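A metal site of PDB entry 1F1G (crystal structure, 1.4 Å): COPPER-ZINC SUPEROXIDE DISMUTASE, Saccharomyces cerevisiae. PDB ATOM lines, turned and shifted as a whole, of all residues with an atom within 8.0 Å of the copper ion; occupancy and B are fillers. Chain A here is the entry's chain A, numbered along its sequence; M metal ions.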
ATOM      1  N   GLY A  45     -15.604 -16.796   7.053  1.00  0.00           N
ATOM      2  CA  GLY A  45     -14.600 -17.148   6.046  1.00  0.00           C
ATOM      3  C   GLY A  45     -14.856 -18.534   5.469  1.00  0.00           C
ATOM      4  O   GLY A  45     -15.258 -19.464   6.160  1.00  0.00           O
ATOM      5  N   PHE A  46     -14.580 -18.676   4.165  1.00  0.00           N
ATOM      6  CA  PHE A  46     -14.993 -19.872   3.443  1.00  0.00           C
ATOM      7  C   PHE A  46     -13.916 -20.173   2.397  1.00  0.00           C
ATOM      8  O   PHE A  46     -13.677 -19.324   1.517  1.00  0.00           O
ATOM      9  CB  PHE A  46     -16.329 -19.576   2.805  1.00  0.00           C
ATOM     10  CG  PHE A  46     -17.058 -20.688   2.114  1.00  0.00           C
ATOM     11  CD1 PHE A  46     -17.258 -21.904   2.702  1.00  0.00           C
ATOM     12  CD2 PHE A  46     -17.573 -20.445   0.825  1.00  0.00           C
ATOM     13  CE1 PHE A  46     -17.962 -22.931   2.069  1.00  0.00           C
ATOM     14  CE2 PHE A  46     -18.288 -21.436   0.208  1.00  0.00           C
ATOM     15  CZ  PHE A  46     -18.482 -22.653   0.809  1.00  0.00           C
ATOM     16  N   HIS A  47     -13.196 -21.311   2.532  1.00  0.00           N
ATOM     17  CA  HIS A  47     -12.077 -21.536   1.607  1.00  0.00           C
ATOM     18  C   HIS A  47     -11.919 -23.015   1.289  1.00  0.00           C
ATOM     19  O   HIS A  47     -12.280 -23.898   2.036  1.00  0.00           O
ATOM     20  CB  HIS A  47     -10.701 -21.095   2.139  1.00  0.00           C
ATOM     21  CG  HIS A  47     -10.749 -19.869   3.003  1.00  0.00           C
ATOM     22  ND1 HIS A  47     -10.678 -19.989   4.356  1.00  0.00           N
ATOM     23  CD2 HIS A  47     -10.919 -18.564   2.708  1.00  0.00           C
ATOM     24  CE1 HIS A  47     -10.782 -18.772   4.838  1.00  0.00           C
ATOM     25  NE2 HIS A  47     -10.931 -17.859   3.904  1.00  0.00           N
ATOM     26  N   ILE A  48     -11.249 -23.236   0.145  1.00  0.00           N
ATOM     27  CA  ILE A  48     -10.713 -24.547  -0.173  1.00  0.00           C
ATOM     28  C   ILE A  48      -9.314 -24.657   0.435  1.00  0.00           C
ATOM     29  O   ILE A  48      -8.481 -23.798   0.184  1.00  0.00           O
ATOM     30  CB  ILE A  48     -10.681 -24.784  -1.699  1.00  0.00           C
ATOM     31  CG1 ILE A  48     -12.054 -24.505  -2.305  1.00  0.00           C
ATOM     32  CG2 ILE A  48     -10.167 -26.173  -1.990  1.00  0.00           C
ATOM     33  CD1 ILE A  48     -12.253 -24.714  -3.782  1.00  0.00           C
ATOM     34  N   HIS A  49      -9.127 -25.695   1.231  1.00  0.00           N
ATOM     35  CA  HIS A  49      -7.810 -25.951   1.825  1.00  0.00           C
ATOM     36  C   HIS A  49      -7.131 -27.078   1.055  1.00  0.00           C
ATOM     37  O   HIS A  49      -7.737 -27.838   0.312  1.00  0.00           O
ATOM     38  CB  HIS A  49      -7.996 -26.267   3.314  1.00  0.00           C
ATOM     39  CG  HIS A  49      -8.330 -25.074   4.131  1.00  0.00           C
ATOM     40  ND1 HIS A  49      -7.568 -24.657   5.202  1.00  0.00           N
ATOM     41  CD2 HIS A  49      -9.336 -24.154   4.057  1.00  0.00           C
ATOM     42  CE1 HIS A  49      -8.127 -23.577   5.731  1.00  0.00           C
ATOM     43  NE2 HIS A  49      -9.192 -23.207   5.066  1.00  0.00           N
ATOM     44  N   ALA A  61      -6.627 -30.582   7.125  1.00  0.00           N
ATOM     45  CA  ALA A  61      -6.904 -29.973   5.825  1.00  0.00           C
ATOM     46  C   ALA A  61      -5.749 -29.079   5.386  1.00  0.00           C
ATOM     47  O   ALA A  61      -5.630 -28.735   4.213  1.00  0.00           O
ATOM     48  CB  ALA A  61      -8.215 -29.236   5.849  1.00  0.00           C
ATOM     49  N   GLY A  62      -4.871 -28.696   6.352  1.00  0.00           N
ATOM     50  CA  GLY A  62      -3.761 -27.852   5.891  1.00  0.00           C
ATOM     51  C   GLY A  62      -4.167 -26.437   5.654  1.00  0.00           C
ATOM     52  O   GLY A  62      -5.243 -25.973   6.061  1.00  0.00           O
ATOM     53  N   PRO A  63      -3.319 -25.665   4.957  1.00  0.00           N
ATOM     54  CA  PRO A  63      -3.569 -24.265   4.661  1.00  0.00           C
ATOM     55  C   PRO A  63      -4.487 -24.034   3.468  1.00  0.00           C
ATOM     56  O   PRO A  63      -4.931 -24.993   2.851  1.00  0.00           O
ATOM     57  CB  PRO A  63      -2.133 -23.768   4.345  1.00  0.00           C
ATOM     58  CG  PRO A  63      -1.551 -24.941   3.617  1.00  0.00           C
ATOM     59  CD  PRO A  63      -2.038 -26.144   4.381  1.00  0.00           C
ATOM     60  N   HIS A  64      -4.774 -22.778   3.145  1.00  0.00           N
ATOM     61  CA  HIS A  64      -5.562 -22.478   1.951  1.00  0.00           C
ATOM     62  C   HIS A  64      -4.864 -23.069   0.723  1.00  0.00           C
ATOM     63  O   HIS A  64      -3.632 -23.001   0.616  1.00  0.00           O
ATOM     64  CB  HIS A  64      -5.728 -20.977   1.741  1.00  0.00           C
ATOM     65  CG  HIS A  64      -6.451 -20.293   2.871  1.00  0.00           C
ATOM     66  ND1 HIS A  64      -6.882 -19.007   2.847  1.00  0.00           N
ATOM     67  CD2 HIS A  64      -6.847 -20.818   4.081  1.00  0.00           C
ATOM     68  CE1 HIS A  64      -7.487 -18.683   3.985  1.00  0.00           C
ATOM     69  NE2 HIS A  64      -7.459 -19.795   4.732  1.00  0.00           N
ATOM     70  N   PHE A  65      -5.626 -23.634  -0.189  1.00  0.00           N
ATOM     71  CA  PHE A  65      -5.080 -24.157  -1.433  1.00  0.00           C
ATOM     72  C   PHE A  65      -4.506 -23.017  -2.251  1.00  0.00           C
ATOM     73  O   PHE A  65      -5.191 -22.055  -2.582  1.00  0.00           O
ATOM     74  CB  PHE A  65      -6.202 -24.898  -2.173  1.00  0.00           C
ATOM     75  CG  PHE A  65      -5.719 -25.528  -3.475  1.00  0.00           C
ATOM     76  CD1 PHE A  65      -4.528 -26.226  -3.541  1.00  0.00           C
ATOM     77  CD2 PHE A  65      -6.492 -25.379  -4.627  1.00  0.00           C
ATOM     78  CE1 PHE A  65      -4.101 -26.765  -4.738  1.00  0.00           C
ATOM     79  CE2 PHE A  65      -6.081 -25.945  -5.827  1.00  0.00           C
ATOM     80  CZ  PHE A  65      -4.897 -26.657  -5.867  1.00  0.00           C
ATOM     81  N   HIS A  72      -3.186 -14.275   0.409  1.00  0.00           N
ATOM     82  CA  HIS A  72      -4.608 -14.375   0.642  1.00  0.00           C
ATOM     83  C   HIS A  72      -5.358 -13.131   0.193  1.00  0.00           C
ATOM     84  O   HIS A  72      -4.916 -12.000   0.496  1.00  0.00           O
ATOM     85  CB  HIS A  72      -4.794 -14.607   2.162  1.00  0.00           C
ATOM     86  CG  HIS A  72      -6.253 -14.782   2.485  1.00  0.00           C
ATOM     87  ND1 HIS A  72      -6.957 -15.949   2.240  1.00  0.00           N
ATOM     88  CD2 HIS A  72      -7.106 -13.856   3.014  1.00  0.00           C
ATOM     89  CE1 HIS A  72      -8.214 -15.699   2.629  1.00  0.00           C
ATOM     90  NE2 HIS A  72      -8.340 -14.452   3.116  1.00  0.00           N
ATOM     91  N   GLY A  83      -7.926 -21.221  -3.430  1.00  0.00           N
ATOM     92  CA  GLY A  83      -9.048 -21.634  -2.597  1.00  0.00           C
ATOM     93  C   GLY A  83      -9.819 -20.486  -1.954  1.00  0.00           C
ATOM     94  O   GLY A  83     -10.760 -20.840  -1.216  1.00  0.00           O
ATOM     95  N   ASP A  84      -9.538 -19.219  -2.160  1.00  0.00           N
ATOM     96  CA  ASP A  84     -10.195 -18.132  -1.434  1.00  0.00           C
ATOM     97  C   ASP A  84     -11.617 -17.907  -1.951  1.00  0.00           C
ATOM     98  O   ASP A  84     -11.832 -17.490  -3.092  1.00  0.00           O
ATOM     99  CB  ASP A  84      -9.366 -16.855  -1.538  1.00  0.00           C
ATOM    100  CG  ASP A  84      -8.100 -16.948  -0.701  1.00  0.00           C
ATOM    101  OD1 ASP A  84      -8.025 -17.824   0.170  1.00  0.00           O
ATOM    102  OD2 ASP A  84      -7.197 -16.130  -0.965  1.00  0.00           O
ATOM    103  N   MET A  85     -12.616 -18.165  -1.100  1.00  0.00           N
ATOM    104  CA  MET A  85     -14.005 -17.972  -1.453  1.00  0.00           C
ATOM    105  C   MET A  85     -14.652 -16.881  -0.584  1.00  0.00           C
ATOM    106  O   MET A  85     -15.862 -16.773  -0.567  1.00  0.00           O
ATOM    107  CB  MET A  85     -14.845 -19.278  -1.395  1.00  0.00           C
ATOM    108  CG  MET A  85     -14.212 -20.363  -2.280  1.00  0.00           C
ATOM    109  SD  MET A  85     -15.230 -21.867  -2.366  1.00  0.00           S
ATOM    110  CE  MET A  85     -15.002 -22.495  -0.684  1.00  0.00           C
ATOM    111  N   GLY A  86     -13.830 -16.051   0.055  1.00  0.00           N
ATOM    112  CA  GLY A  86     -14.289 -14.897   0.763  1.00  0.00           C
ATOM    113  C   GLY A  86     -15.146 -15.201   1.982  1.00  0.00           C
ATOM    114  O   GLY A  86     -14.873 -16.168   2.712  1.00  0.00           O
ATOM    115  N   SER A 117     -10.187 -30.026   0.509  1.00  0.00           N
ATOM    116  CA  SER A 117     -11.239 -29.842   1.509  1.00  0.00           C
ATOM    117  C   SER A 117     -11.875 -28.481   1.400  1.00  0.00           C
ATOM    118  O   SER A 117     -11.243 -27.510   0.972  1.00  0.00           O
ATOM    119  CB  SER A 117     -10.645 -29.930   2.938  1.00  0.00           C
ATOM    120  OG  SER A 117     -10.256 -31.222   3.264  1.00  0.00           O
ATOM    121  N   VAL A 118     -13.131 -28.393   1.900  1.00  0.00           N
ATOM    122  CA  VAL A 118     -13.736 -27.090   2.140  1.00  0.00           C
ATOM    123  C   VAL A 118     -13.780 -26.859   3.655  1.00  0.00           C
ATOM    124  O   VAL A 118     -14.092 -27.804   4.350  1.00  0.00           O
ATOM    125  CB  VAL A 118     -15.194 -27.018   1.612  1.00  0.00           C
ATOM    126  CG1 VAL A 118     -15.816 -25.717   1.993  1.00  0.00           C
ATOM    127  CG2 VAL A 118     -15.197 -27.246   0.119  1.00  0.00           C
ATOM    128  N   VAL A 119     -13.464 -25.639   4.049  1.00  0.00           N
ATOM    129  CA  VAL A 119     -13.543 -25.270   5.467  1.00  0.00           C
ATOM    130  C   VAL A 119     -14.429 -24.039   5.567  1.00  0.00           C
ATOM    131  O   VAL A 119     -14.302 -23.088   4.819  1.00  0.00           O
ATOM    132  CB  VAL A 119     -12.140 -24.973   6.052  1.00  0.00           C
ATOM    133  CG1 VAL A 119     -12.218 -24.495   7.503  1.00  0.00           C
ATOM    134  CG2 VAL A 119     -11.233 -26.186   5.928  1.00  0.00           C
ATOM    135  N   ILE A 120     -15.357 -24.110   6.566  1.00  0.00           N
ATOM    136  CA  ILE A 120     -16.077 -22.916   6.992  1.00  0.00           C
ATOM    137  C   ILE A 120     -15.541 -22.460   8.362  1.00  0.00           C
ATOM    138  O   ILE A 120     -15.335 -23.323   9.211  1.00  0.00           O
ATOM    139  CB  ILE A 120     -17.599 -23.188   7.054  1.00  0.00           C
ATOM    140  CG1 ILE A 120     -18.430 -21.988   7.487  1.00  0.00           C
ATOM    141  CG2 ILE A 120     -17.898 -24.429   7.906  1.00  0.00           C
ATOM    142  CD1 ILE A 120     -18.419 -20.814   6.545  1.00  0.00           C
ATOM    143  N   HIS A 121     -15.318 -21.169   8.476  1.00  0.00           N
ATOM    144  CA  HIS A 121     -14.635 -20.618   9.651  1.00  0.00           C
ATOM    145  C   HIS A 121     -15.637 -20.001  10.617  1.00  0.00           C
ATOM    146  O   HIS A 121     -16.773 -19.700  10.318  1.00  0.00           O
ATOM    147  CB  HIS A 121     -13.595 -19.550   9.227  1.00  0.00           C
ATOM    148  CG  HIS A 121     -12.420 -20.189   8.561  1.00  0.00           C
ATOM    149  ND1 HIS A 121     -11.282 -20.597   9.235  1.00  0.00           N
ATOM    150  CD2 HIS A 121     -12.194 -20.496   7.259  1.00  0.00           C
ATOM    151  CE1 HIS A 121     -10.426 -21.136   8.360  1.00  0.00           C
ATOM    152  NE2 HIS A 121     -10.947 -21.088   7.128  1.00  0.00           N
ATOM    153  N   ASP A 125     -13.456 -13.321   7.399  1.00  0.00           N
ATOM    154  CA  ASP A 125     -12.229 -13.199   6.609  1.00  0.00           C
ATOM    155  C   ASP A 125     -11.969 -11.743   6.288  1.00  0.00           C
ATOM    156  O   ASP A 125     -12.844 -11.108   5.720  1.00  0.00           O
ATOM    157  CB  ASP A 125     -12.448 -14.033   5.339  1.00  0.00           C
ATOM    158  CG  ASP A 125     -11.298 -14.150   4.377  1.00  0.00           C
ATOM    159  OD1 ASP A 125     -10.427 -13.267   4.377  1.00  0.00           O
ATOM    160  OD2 ASP A 125     -11.297 -15.119   3.596  1.00  0.00           O
ATOM    161  N   LYS A 137      -2.151 -14.567   5.034  1.00  0.00           N
ATOM    162  CA  LYS A 137      -2.058 -16.009   5.072  1.00  0.00           C
ATOM    163  C   LYS A 137      -3.464 -16.646   5.165  1.00  0.00           C
ATOM    164  O   LYS A 137      -3.818 -17.527   4.371  1.00  0.00           O
ATOM    165  CB  LYS A 137      -1.140 -16.513   6.179  1.00  0.00           C
ATOM    166  CG  LYS A 137       0.330 -16.227   5.924  1.00  0.00           C
ATOM    167  CD  LYS A 137       0.778 -14.852   5.522  1.00  0.00           C
ATOM    168  CE  LYS A 137       1.939 -14.305   6.306  1.00  0.00           C
ATOM    169  NZ  LYS A 137       2.353 -12.946   5.849  1.00  0.00           N
ATOM    170  N   THR A 138      -4.232 -16.160   6.135  1.00  0.00           N
ATOM    171  CA  THR A 138      -5.517 -16.739   6.450  1.00  0.00           C
ATOM    172  C   THR A 138      -6.682 -15.774   6.401  1.00  0.00           C
ATOM    173  O   THR A 138      -7.814 -16.183   6.636  1.00  0.00           O
ATOM    174  CB  THR A 138      -5.518 -17.299   7.902  1.00  0.00           C
ATOM    175  OG1 THR A 138      -5.316 -16.179   8.764  1.00  0.00           O
ATOM    176  CG2 THR A 138      -4.378 -18.295   8.102  1.00  0.00           C
ATOM    177  N   ALA A 141      -9.458 -15.407   9.613  1.00  0.00           N
ATOM    178  CA  ALA A 141     -10.797 -15.927   9.717  1.00  0.00           C
ATOM    179  C   ALA A 141     -10.996 -16.861  10.916  1.00  0.00           C
ATOM    180  O   ALA A 141     -12.119 -17.321  11.173  1.00  0.00           O
ATOM    181  CB  ALA A 141     -11.178 -16.702   8.466  1.00  0.00           C
ATOM    182  N   GLY A 142      -9.918 -17.162  11.644  1.00  0.00           N
ATOM    183  CA  GLY A 142     -10.059 -17.917  12.870  1.00  0.00           C
ATOM    184  C   GLY A 142     -10.336 -19.374  12.791  1.00  0.00           C
ATOM    185  O   GLY A 142      -9.978 -20.090  11.839  1.00  0.00           O
ATOM    186  N   PRO A 143     -10.985 -19.943  13.811  1.00  0.00           N
ATOM    187  CA  PRO A 143     -11.225 -21.376  13.928  1.00  0.00           C
ATOM    188  C   PRO A 143     -11.992 -22.033  12.744  1.00  0.00           C
ATOM    189  O   PRO A 143     -12.630 -21.312  11.994  1.00  0.00           O
ATOM    190  CB  PRO A 143     -12.051 -21.497  15.211  1.00  0.00           C
ATOM    191  CG  PRO A 143     -11.637 -20.272  15.998  1.00  0.00           C
ATOM    192  CD  PRO A 143     -11.444 -19.159  14.989  1.00  0.00           C
ATOM    193  N   ARG A 144     -11.864 -23.347  12.737  1.00  0.00           N
ATOM    194  CA  ARG A 144     -12.441 -24.189  11.660  1.00  0.00           C
ATOM    195  C   ARG A 144     -13.539 -25.086  12.244  1.00  0.00           C
ATOM    196  O   ARG A 144     -13.327 -26.260  12.484  1.00  0.00           O
ATOM    197  CB  ARG A 144     -11.376 -25.066  11.034  1.00  0.00           C
ATOM    198  CG  ARG A 144     -10.160 -24.246  10.528  1.00  0.00           C
ATOM    199  CD  ARG A 144      -9.131 -25.213   9.943  1.00  0.00           C
ATOM    200  NE  ARG A 144      -7.973 -24.417   9.478  1.00  0.00           N
ATOM    201  CZ  ARG A 144      -6.997 -24.988   8.764  1.00  0.00           C
ATOM    202  NH1 ARG A 144      -6.983 -26.277   8.436  1.00  0.00           N
ATOM    203  NH2 ARG A 144      -5.987 -24.190   8.377  1.00  0.00           N
ATOM    204  N   ALA A 146     -16.120 -26.485  10.923  1.00  0.00           N
ATOM    205  CA  ALA A 146     -16.558 -27.616  10.092  1.00  0.00           C
ATOM    206  C   ALA A 146     -15.743 -27.611   8.766  1.00  0.00           C
ATOM    207  O   ALA A 146     -15.262 -26.575   8.367  1.00  0.00           O
ATOM    208  CB  ALA A 146     -18.024 -27.602   9.806  1.00  0.00           C
HETATM  209 CU    CU M   1     -10.224 -21.597   5.354  1.00  0.00          CU
HETATM  210 ZN    ZN M   2      -6.520 -17.700   1.398  1.00  0.00          ZN
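The backbone NH (N) of His 121 sits at hydrogen-bond distance from the backbone carbonyl oxygen (O) of Gly 45 (2.9 Å).
A ring nitrogen (ND1) of His 47 lies close to a ring nitrogen (NE2) of His 64 (3.2 Å).
A ring nitrogen (ND1) of His 121 sits at hydrogen-bond distance from the backbone carbonyl oxygen (O) of Gly 142, at 3.0 Å.
O of His 47 sits at hydrogen-bond distance from N of Val 119.
The backbone carbonyl oxygen (O) of Ser 117 lies within hydrogen-bond range of the backbone NH (N) of His 49 (2.8 Å).
The side-chain carboxylate (OD2) of Asp 125 sits at hydrogen-bond distance from a ring nitrogen (NE2) of His 47, 2.8 Å away.
The backbone carbonyl oxygen (O) of Pro 143 sits at hydrogen-bond distance from a ring nitrogen (ND1) of His 121.
ND1 of His 49 is in hydrogen-bond range of O of Gly 62 (2.8 Å).
The copper ion is bound by NE2 of His 49 (1.9 Å).
A ring nitrogen (ND1) of His 47 is bound to the copper ion (1.9 Å).
The copper ion is bound by a ring nitrogen (NE2) of His 121 (2.0 Å).
The copper ion has three donor atoms within binding distance.
Merely in contact with the copper ion: His 64 and Val 119.
Five residues have an atom within 4 Å of the copper ion: His 47, His 49, His 64, Val 119 and His 121.
Along chain A the residues within 4 Å of the copper ion span positions 47 to 121.
The nearest printed residue that does not touch the copper ion is Phe 46 (4.9 Å).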
